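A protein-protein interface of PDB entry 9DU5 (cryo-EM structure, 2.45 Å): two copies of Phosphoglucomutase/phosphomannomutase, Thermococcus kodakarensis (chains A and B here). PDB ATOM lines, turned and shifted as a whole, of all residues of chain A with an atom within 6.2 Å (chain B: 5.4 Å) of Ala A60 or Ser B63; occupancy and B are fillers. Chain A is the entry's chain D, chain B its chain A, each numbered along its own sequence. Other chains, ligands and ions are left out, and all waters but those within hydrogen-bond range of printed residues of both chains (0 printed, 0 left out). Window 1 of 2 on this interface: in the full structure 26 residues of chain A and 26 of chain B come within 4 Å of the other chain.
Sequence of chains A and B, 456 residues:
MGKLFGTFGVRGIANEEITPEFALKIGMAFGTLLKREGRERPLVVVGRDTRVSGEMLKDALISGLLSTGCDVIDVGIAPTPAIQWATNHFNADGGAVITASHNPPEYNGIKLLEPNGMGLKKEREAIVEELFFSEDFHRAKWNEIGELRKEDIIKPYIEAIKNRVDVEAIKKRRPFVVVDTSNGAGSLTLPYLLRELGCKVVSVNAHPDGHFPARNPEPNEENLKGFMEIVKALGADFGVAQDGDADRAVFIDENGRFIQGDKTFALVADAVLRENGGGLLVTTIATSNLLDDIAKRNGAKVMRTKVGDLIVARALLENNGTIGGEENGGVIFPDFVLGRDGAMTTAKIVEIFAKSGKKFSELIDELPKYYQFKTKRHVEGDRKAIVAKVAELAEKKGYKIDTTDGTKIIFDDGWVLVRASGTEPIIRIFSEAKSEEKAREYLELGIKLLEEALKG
Of the 18 printed residues of chain A, 7 touch a printed residue of chain B.
Hydrophobic or aromatic side chains of chain A within 4 Å of the printed part of chain B: Pro A20, Met A56, Ala A60 and Ile A62.
Printed residues of chain B that touch a printed residue of chain A: Leu B24, Asp B59, Ala B60, Ile B62, Ser B63, Leu B66 and Ser B67.
Hydrophobic or aromatic side chains of chain B within 4 Å of the printed part of chain A: Leu B24, Ala B60, Ile B62 and Leu B66.
Among the printed residues, merely in contact across the chains: Pro A20 with Leu B24 (3.6 Å), Pro A20 with Ser B63 (3.4 Å), Pro A20 with Ser B67 (3.5 Å), Glu A21 with Leu B24 (3.5 Å), Met A56 with Leu B66 (3.8 Å), Met A56 with Ser B67 (3.6 Å), Asp A59 with Asp B59 (3.8 Å), Asp A59 with Ile B62 (3.6 Å), Asp A59 with Ser B63 (3.8 Å), Ala A60 with Ser B63 (3.2 Å), Ile A62 with Asp B59 (3.7 Å), Ser A63 with Asp B59 (3.9 Å) and Ser A63 with Ala B60 (3.3 Å).
The side-chain hydroxyl (OG) of Ser B63 is in hydrogen-bond range of the backbone carbonyl oxygen (O) of Met A56, at 2.8 Å.
Asp A59 touches its own counterpart, Asp B59.
Asp A59 touches Ile B62, and with the chains exchanged Ile A62 touches Asp B59.
Asp A59 touches Ser B63, and with the chains exchanged Ser A63 touches Asp B59.
Ala A60 touches Ser B63, and with the chains exchanged Ser A63 touches Ala B60.
Positions printed for both chains: 24, 58, 59, 60, 61, 62, 63, 64 and 65.
OD1 of Asp B59 is in salt-bridge range of NZ of Lys B58, 3.5 Å away.
OG of Ser B67 lies within hydrogen-bond range of O of Gly B64 (2.8 Å).
OD1 of Asp A59 is in salt-bridge range of NZ of Lys A58.
Of the printed residues of chain B, Glu A21 touches Leu B24.
Printed residues of chain B within 4 Å of Met A56: Ser B63 (2.8 Å), Leu B66 (3.8 Å) and Ser B67 (3.6 Å).
Ala A60 touches just one residue of chain B: Ser B63.
Printed residues of chain A within 4 Å of Ala B60: Ser A63 (3.3 Å).
Of the printed residues of chain A, Ile B62 touches Asp A59.
Ser B63 touches just these residues of chain A: Pro A20 (3.4 Å), Met A56 (2.8 Å), Asp A59 (3.8 Å) and Ala A60 (3.2 Å).
The nearest residue of chain B that does not touch Ala A60 is Leu B24 (4.6 Å).
The nearest residue of chain A that does not touch Ser B63 is Leu A57 (4.7 Å).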
ATOM      1  N   THR A  19     -17.399 -20.490  -9.445  1.00  0.00           N
ATOM      2  CA  THR A  19     -18.345 -20.083 -10.469  1.00  0.00           C
ATOM      3  C   THR A  19     -19.268 -18.999  -9.932  1.00  0.00           C
ATOM      4  O   THR A  19     -19.357 -18.793  -8.718  1.00  0.00           O
ATOM      5  CB  THR A  19     -19.160 -21.289 -10.933  1.00  0.00           C
ATOM      6  OG1 THR A  19     -19.737 -21.945  -9.798  1.00  0.00           O
ATOM      7  CG2 THR A  19     -18.277 -22.269 -11.677  1.00  0.00           C
ATOM      8  N   PRO A  20     -19.956 -18.265 -10.810  1.00  0.00           N
ATOM      9  CA  PRO A  20     -20.955 -17.302 -10.324  1.00  0.00           C
ATOM     10  C   PRO A  20     -22.045 -17.934  -9.480  1.00  0.00           C
ATOM     11  O   PRO A  20     -22.555 -17.276  -8.567  1.00  0.00           O
ATOM     12  CB  PRO A  20     -21.515 -16.710 -11.621  1.00  0.00           C
ATOM     13  CG  PRO A  20     -20.361 -16.784 -12.543  1.00  0.00           C
ATOM     14  CD  PRO A  20     -19.776 -18.141 -12.266  1.00  0.00           C
ATOM     15  N   GLU A  21     -22.419 -19.185  -9.751  1.00  0.00           N
ATOM     16  CA  GLU A  21     -23.328 -19.894  -8.859  1.00  0.00           C
ATOM     17  C   GLU A  21     -22.724 -20.075  -7.474  1.00  0.00           C
ATOM     18  O   GLU A  21     -23.420 -19.893  -6.470  1.00  0.00           O
ATOM     19  CB  GLU A  21     -23.694 -21.256  -9.449  1.00  0.00           C
ATOM     20  CG  GLU A  21     -24.130 -21.206 -10.900  1.00  0.00           C
ATOM     21  CD  GLU A  21     -23.075 -21.742 -11.845  1.00  0.00           C
ATOM     22  OE1 GLU A  21     -23.047 -22.968 -12.075  1.00  0.00           O
ATOM     23  OE2 GLU A  21     -22.272 -20.935 -12.359  1.00  0.00           O
ATOM     24  N   ALA A  23     -20.376 -18.158  -6.031  1.00  0.00           N
ATOM     25  CA  ALA A  23     -20.341 -16.859  -5.368  1.00  0.00           C
ATOM     26  C   ALA A  23     -21.728 -16.420  -4.922  1.00  0.00           C
ATOM     27  O   ALA A  23     -21.882 -15.851  -3.836  1.00  0.00           O
ATOM     28  CB  ALA A  23     -19.725 -15.811  -6.292  1.00  0.00           C
ATOM     29  N   LEU A  24     -22.746 -16.671  -5.746  1.00  0.00           N
ATOM     30  CA  LEU A  24     -24.115 -16.335  -5.375  1.00  0.00           C
ATOM     31  C   LEU A  24     -24.559 -17.117  -4.147  1.00  0.00           C
ATOM     32  O   LEU A  24     -25.175 -16.560  -3.232  1.00  0.00           O
ATOM     33  CB  LEU A  24     -25.044 -16.608  -6.554  1.00  0.00           C
ATOM     34  CG  LEU A  24     -26.523 -16.268  -6.401  1.00  0.00           C
ATOM     35  CD1 LEU A  24     -26.744 -14.774  -6.476  1.00  0.00           C
ATOM     36  CD2 LEU A  24     -27.306 -16.973  -7.475  1.00  0.00           C
ATOM     37  N   LYS A  25     -24.255 -18.417  -4.109  1.00  0.00           N
ATOM     38  CA  LYS A  25     -24.613 -19.226  -2.950  1.00  0.00           C
ATOM     39  C   LYS A  25     -23.849 -18.796  -1.706  1.00  0.00           C
ATOM     40  O   LYS A  25     -24.412 -18.801  -0.607  1.00  0.00           O
ATOM     41  CB  LYS A  25     -24.364 -20.704  -3.246  1.00  0.00           C
ATOM     42  CG  LYS A  25     -25.398 -21.335  -4.158  1.00  0.00           C
ATOM     43  CD  LYS A  25     -25.114 -22.810  -4.375  1.00  0.00           C
ATOM     44  CE  LYS A  25     -25.037 -23.556  -3.058  1.00  0.00           C
ATOM     45  NZ  LYS A  25     -24.847 -25.019  -3.257  1.00  0.00           N
ATOM     46  N   GLY A  27     -22.792 -15.718  -1.084  1.00  0.00           N
ATOM     47  CA  GLY A  27     -23.423 -14.484  -0.650  1.00  0.00           C
ATOM     48  C   GLY A  27     -24.752 -14.720   0.039  1.00  0.00           C
ATOM     49  O   GLY A  27     -25.052 -14.095   1.059  1.00  0.00           O
ATOM     50  N   GLU A  55     -14.998  -9.195 -11.032  1.00  0.00           N
ATOM     51  CA  GLU A  55     -16.179  -8.359 -11.218  1.00  0.00           C
ATOM     52  C   GLU A  55     -17.448  -9.200 -11.303  1.00  0.00           C
ATOM     53  O   GLU A  55     -18.455  -8.875 -10.665  1.00  0.00           O
ATOM     54  CB  GLU A  55     -16.021  -7.493 -12.465  1.00  0.00           C
ATOM     55  CG  GLU A  55     -17.235  -6.636 -12.774  1.00  0.00           C
ATOM     56  CD  GLU A  55     -16.869  -5.193 -13.061  1.00  0.00           C
ATOM     57  OE1 GLU A  55     -16.084  -4.953 -14.002  1.00  0.00           O
ATOM     58  OE2 GLU A  55     -17.365  -4.298 -12.343  1.00  0.00           O
ATOM     59  N   MET A  56     -17.423 -10.283 -12.084  1.00  0.00           N
ATOM     60  CA  MET A  56     -18.590 -11.156 -12.163  1.00  0.00           C
ATOM     61  C   MET A  56     -18.841 -11.864 -10.836  1.00  0.00           C
ATOM     62  O   MET A  56     -19.994 -12.024 -10.416  1.00  0.00           O
ATOM     63  CB  MET A  56     -18.419 -12.162 -13.303  1.00  0.00           C
ATOM     64  CG  MET A  56     -17.380 -13.240 -13.051  1.00  0.00           C
ATOM     65  SD  MET A  56     -17.693 -14.770 -13.939  1.00  0.00           S
ATOM     66  CE  MET A  56     -16.527 -15.865 -13.136  1.00  0.00           C
ATOM     67  N   LEU A  57     -17.772 -12.288 -10.159  1.00  0.00           N
ATOM     68  CA  LEU A  57     -17.923 -12.917  -8.855  1.00  0.00           C
ATOM     69  C   LEU A  57     -18.479 -11.939  -7.833  1.00  0.00           C
ATOM     70  O   LEU A  57     -19.343 -12.306  -7.030  1.00  0.00           O
ATOM     71  CB  LEU A  57     -16.580 -13.475  -8.391  1.00  0.00           C
ATOM     72  CG  LEU A  57     -16.129 -14.750  -9.101  1.00  0.00           C
ATOM     73  CD1 LEU A  57     -14.810 -15.227  -8.534  1.00  0.00           C
ATOM     74  CD2 LEU A  57     -17.187 -15.830  -8.988  1.00  0.00           C
ATOM     75  N   LYS A  58     -18.000 -10.694  -7.851  1.00  0.00           N
ATOM     76  CA  LYS A  58     -18.543  -9.677  -6.958  1.00  0.00           C
ATOM     77  C   LYS A  58     -20.012  -9.410  -7.258  1.00  0.00           C
ATOM     78  O   LYS A  58     -20.816  -9.241  -6.339  1.00  0.00           O
ATOM     79  CB  LYS A  58     -17.729  -8.391  -7.073  1.00  0.00           C
ATOM     80  CG  LYS A  58     -18.145  -7.300  -6.108  1.00  0.00           C
ATOM     81  CD  LYS A  58     -18.131  -5.943  -6.786  1.00  0.00           C
ATOM     82  CE  LYS A  58     -18.874  -5.988  -8.111  1.00  0.00           C
ATOM     83  NZ  LYS A  58     -18.942  -4.652  -8.760  1.00  0.00           N
ATOM     84  N   ASP A  59     -20.375  -9.360  -8.542  1.00  0.00           N
ATOM     85  CA  ASP A  59     -21.771  -9.147  -8.902  1.00  0.00           C
ATOM     86  C   ASP A  59     -22.659 -10.272  -8.392  1.00  0.00           C
ATOM     87  O   ASP A  59     -23.724 -10.008  -7.823  1.00  0.00           O
ATOM     88  CB  ASP A  59     -21.907  -9.016 -10.418  1.00  0.00           C
ATOM     89  CG  ASP A  59     -21.771  -7.586 -10.893  1.00  0.00           C
ATOM     90  OD1 ASP A  59     -21.666  -6.682 -10.038  1.00  0.00           O
ATOM     91  OD2 ASP A  59     -21.772  -7.367 -12.121  1.00  0.00           O
ATOM     92  N   ALA A  60     -22.232 -11.523  -8.569  1.00  0.00           N
ATOM     93  CA  ALA A  60     -23.004 -12.652  -8.060  1.00  0.00           C
ATOM     94  C   ALA A  60     -23.110 -12.622  -6.541  1.00  0.00           C
ATOM     95  O   ALA A  60     -24.190 -12.861  -5.986  1.00  0.00           O
ATOM     96  CB  ALA A  60     -22.378 -13.966  -8.521  1.00  0.00           C
ATOM     97  N   LEU A  61     -22.006 -12.324  -5.854  1.00  0.00           N
ATOM     98  CA  LEU A  61     -22.025 -12.275  -4.396  1.00  0.00           C
ATOM     99  C   LEU A  61     -22.953 -11.177  -3.890  1.00  0.00           C
ATOM    100  O   LEU A  61     -23.714 -11.381  -2.939  1.00  0.00           O
ATOM    101  CB  LEU A  61     -20.609 -12.067  -3.866  1.00  0.00           C
ATOM    102  CG  LEU A  61     -20.441 -12.141  -2.351  1.00  0.00           C
ATOM    103  CD1 LEU A  61     -20.020 -13.532  -1.919  1.00  0.00           C
ATOM    104  CD2 LEU A  61     -19.437 -11.109  -1.899  1.00  0.00           C
ATOM    105  N   ILE A  62     -22.896  -9.999  -4.513  1.00  0.00           N
ATOM    106  CA  ILE A  62     -23.746  -8.888  -4.094  1.00  0.00           C
ATOM    107  C   ILE A  62     -25.208  -9.204  -4.368  1.00  0.00           C
ATOM    108  O   ILE A  62     -26.085  -8.906  -3.550  1.00  0.00           O
ATOM    109  CB  ILE A  62     -23.300  -7.586  -4.784  1.00  0.00           C
ATOM    110  CG1 ILE A  62     -21.965  -7.114  -4.210  1.00  0.00           C
ATOM    111  CG2 ILE A  62     -24.356  -6.505  -4.636  1.00  0.00           C
ATOM    112  CD1 ILE A  62     -21.425  -5.870  -4.867  1.00  0.00           C
ATOM    113  N   SER A  63     -25.495  -9.825  -5.516  1.00  0.00           N
ATOM    114  CA  SER A  63     -26.865 -10.232  -5.805  1.00  0.00           C
ATOM    115  C   SER A  63     -27.371 -11.223  -4.767  1.00  0.00           C
ATOM    116  O   SER A  63     -28.530 -11.150  -4.343  1.00  0.00           O
ATOM    117  CB  SER A  63     -26.948 -10.832  -7.206  1.00  0.00           C
ATOM    118  OG  SER A  63     -28.235 -11.365  -7.451  1.00  0.00           O
ATOM    119  N   GLY A  64     -26.518 -12.159  -4.348  1.00  0.00           N
ATOM    120  CA  GLY A  64     -26.909 -13.077  -3.292  1.00  0.00           C
ATOM    121  C   GLY A  64     -27.147 -12.381  -1.966  1.00  0.00           C
ATOM    122  O   GLY A  64     -28.086 -12.714  -1.239  1.00  0.00           O
ATOM    123  N   LEU A  65     -26.296 -11.409  -1.630  1.00  0.00           N
ATOM    124  CA  LEU A  65     -26.451 -10.685  -0.372  1.00  0.00           C
ATOM    125  C   LEU A  65     -27.717  -9.838  -0.366  1.00  0.00           C
ATOM    126  O   LEU A  65     -28.412  -9.760   0.653  1.00  0.00           O
ATOM    127  CB  LEU A  65     -25.223  -9.813  -0.114  1.00  0.00           C
ATOM    128  CG  LEU A  65     -23.991 -10.516   0.454  1.00  0.00           C
ATOM    129  CD1 LEU A  65     -22.755  -9.661   0.252  1.00  0.00           C
ATOM    130  CD2 LEU A  65     -24.186 -10.835   1.923  1.00  0.00           C
ATOM    131  N   LEU B  24     -29.396 -15.598 -12.741  1.00  0.00           N
ATOM    132  CA  LEU B  24     -28.048 -16.014 -13.112  1.00  0.00           C
ATOM    133  C   LEU B  24     -28.082 -17.123 -14.155  1.00  0.00           C
ATOM    134  O   LEU B  24     -27.312 -17.104 -15.122  1.00  0.00           O
ATOM    135  CB  LEU B  24     -27.289 -16.465 -11.868  1.00  0.00           C
ATOM    136  CG  LEU B  24     -25.822 -16.846 -12.043  1.00  0.00           C
ATOM    137  CD1 LEU B  24     -24.939 -15.622 -11.951  1.00  0.00           C
ATOM    138  CD2 LEU B  24     -25.437 -17.859 -10.996  1.00  0.00           C
ATOM    139  N   LYS B  58     -30.686  -7.850 -11.847  1.00  0.00           N
ATOM    140  CA  LYS B  58     -29.776  -7.366 -12.880  1.00  0.00           C
ATOM    141  C   LYS B  58     -28.340  -7.772 -12.577  1.00  0.00           C
ATOM    142  O   LYS B  58     -27.590  -8.153 -13.481  1.00  0.00           O
ATOM    143  CB  LYS B  58     -29.891  -5.849 -13.010  1.00  0.00           C
ATOM    144  CG  LYS B  58     -29.073  -5.256 -14.139  1.00  0.00           C
ATOM    145  CD  LYS B  58     -28.389  -3.974 -13.700  1.00  0.00           C
ATOM    146  CE  LYS B  58     -27.633  -4.178 -12.399  1.00  0.00           C
ATOM    147  NZ  LYS B  58     -26.944  -2.940 -11.952  1.00  0.00           N
ATOM    148  N   ASP B  59     -27.934  -7.688 -11.307  1.00  0.00           N
ATOM    149  CA  ASP B  59     -26.586  -8.098 -10.933  1.00  0.00           C
ATOM    150  C   ASP B  59     -26.365  -9.581 -11.187  1.00  0.00           C
ATOM    151  O   ASP B  59     -25.324  -9.970 -11.728  1.00  0.00           O
ATOM    152  CB  ASP B  59     -26.326  -7.772  -9.464  1.00  0.00           C
ATOM    153  CG  ASP B  59     -25.777  -6.377  -9.266  1.00  0.00           C
ATOM    154  OD1 ASP B  59     -25.512  -5.692 -10.275  1.00  0.00           O
ATOM    155  OD2 ASP B  59     -25.609  -5.967  -8.098  1.00  0.00           O
ATOM    156  N   ALA B  60     -27.339 -10.418 -10.824  1.00  0.00           N
ATOM    157  CA  ALA B  60     -27.221 -11.847 -11.100  1.00  0.00           C
ATOM    158  C   ALA B  60     -27.162 -12.128 -12.597  1.00  0.00           C
ATOM    159  O   ALA B  60     -26.349 -12.944 -13.049  1.00  0.00           O
ATOM    160  CB  ALA B  60     -28.388 -12.600 -10.464  1.00  0.00           C
ATOM    161  N   LEU B  61     -28.008 -11.456 -13.380  1.00  0.00           N
ATOM    162  CA  LEU B  61     -28.022 -11.668 -14.822  1.00  0.00           C
ATOM    163  C   LEU B  61     -26.698 -11.260 -15.455  1.00  0.00           C
ATOM    164  O   LEU B  61     -26.168 -11.964 -16.321  1.00  0.00           O
ATOM    165  CB  LEU B  61     -29.176 -10.889 -15.448  1.00  0.00           C
ATOM    166  CG  LEU B  61     -29.381 -11.073 -16.950  1.00  0.00           C
ATOM    167  CD1 LEU B  61     -30.307 -12.241 -17.233  1.00  0.00           C
ATOM    168  CD2 LEU B  61     -29.911  -9.799 -17.560  1.00  0.00           C
ATOM    169  N   ILE B  62     -26.154 -10.113 -15.042  1.00  0.00           N
ATOM    170  CA  ILE B  62     -24.894  -9.636 -15.603  1.00  0.00           C
ATOM    171  C   ILE B  62     -23.751 -10.556 -15.202  1.00  0.00           C
ATOM    172  O   ILE B  62     -22.865 -10.855 -16.010  1.00  0.00           O
ATOM    173  CB  ILE B  62     -24.638  -8.180 -15.174  1.00  0.00           C
ATOM    174  CG1 ILE B  62     -25.609  -7.241 -15.889  1.00  0.00           C
ATOM    175  CG2 ILE B  62     -23.201  -7.776 -15.454  1.00  0.00           C
ATOM    176  CD1 ILE B  62     -25.424  -5.788 -15.536  1.00  0.00           C
ATOM    177  N   SER B  63     -23.755 -11.030 -13.954  1.00  0.00           N
ATOM    178  CA  SER B  63     -22.738 -11.986 -13.533  1.00  0.00           C
ATOM    179  C   SER B  63     -22.808 -13.259 -14.364  1.00  0.00           C
ATOM    180  O   SER B  63     -21.774 -13.818 -14.744  1.00  0.00           O
ATOM    181  CB  SER B  63     -22.897 -12.305 -12.049  1.00  0.00           C
ATOM    182  OG  SER B  63     -22.048 -13.371 -11.671  1.00  0.00           O
ATOM    183  N   GLY B  64     -24.020 -13.734 -14.653  1.00  0.00           N
ATOM    184  CA  GLY B  64     -24.157 -14.896 -15.515  1.00  0.00           C
ATOM    185  C   GLY B  64     -23.680 -14.637 -16.933  1.00  0.00           C
ATOM    186  O   GLY B  64     -23.062 -15.503 -17.556  1.00  0.00           O
ATOM    187  N   LEU B  65     -23.965 -13.446 -17.462  1.00  0.00           N
ATOM    188  CA  LEU B  65     -23.564 -13.121 -18.828  1.00  0.00           C
ATOM    189  C   LEU B  65     -22.053 -12.974 -18.948  1.00  0.00           C
ATOM    190  O   LEU B  65     -21.463 -13.390 -19.951  1.00  0.00           O
ATOM    191  CB  LEU B  65     -24.263 -11.842 -19.289  1.00  0.00           C
ATOM    192  CG  LEU B  65     -25.656 -11.986 -19.901  1.00  0.00           C
ATOM    193  CD1 LEU B  65     -26.394 -10.662 -19.843  1.00  0.00           C
ATOM    194  CD2 LEU B  65     -25.575 -12.493 -21.327  1.00  0.00           C
ATOM    195  N   LEU B  66     -21.411 -12.373 -17.944  1.00  0.00           N
ATOM    196  CA  LEU B  66     -19.964 -12.190 -17.994  1.00  0.00           C
ATOM    197  C   LEU B  66     -19.225 -13.518 -17.928  1.00  0.00           C
ATOM    198  O   LEU B  66     -18.154 -13.660 -18.530  1.00  0.00           O
ATOM    199  CB  LEU B  66     -19.508 -11.277 -16.857  1.00  0.00           C
ATOM    200  CG  LEU B  66     -19.974  -9.822 -16.893  1.00  0.00           C
ATOM    201  CD1 LEU B  66     -19.384  -9.045 -15.732  1.00  0.00           C
ATOM    202  CD2 LEU B  66     -19.618  -9.169 -18.211  1.00  0.00           C
ATOM    203  N   SER B  67     -19.772 -14.498 -17.205  1.00  0.00           N
ATOM    204  CA  SER B  67     -19.125 -15.799 -17.092  1.00  0.00           C
ATOM    205  C   SER B  67     -19.084 -16.546 -18.416  1.00  0.00           C
ATOM    206  O   SER B  67     -18.238 -17.429 -18.587  1.00  0.00           O
ATOM    207  CB  SER B  67     -19.842 -16.651 -16.048  1.00  0.00           C
ATOM    208  OG  SER B  67     -21.058 -17.163 -16.557  1.00  0.00           O
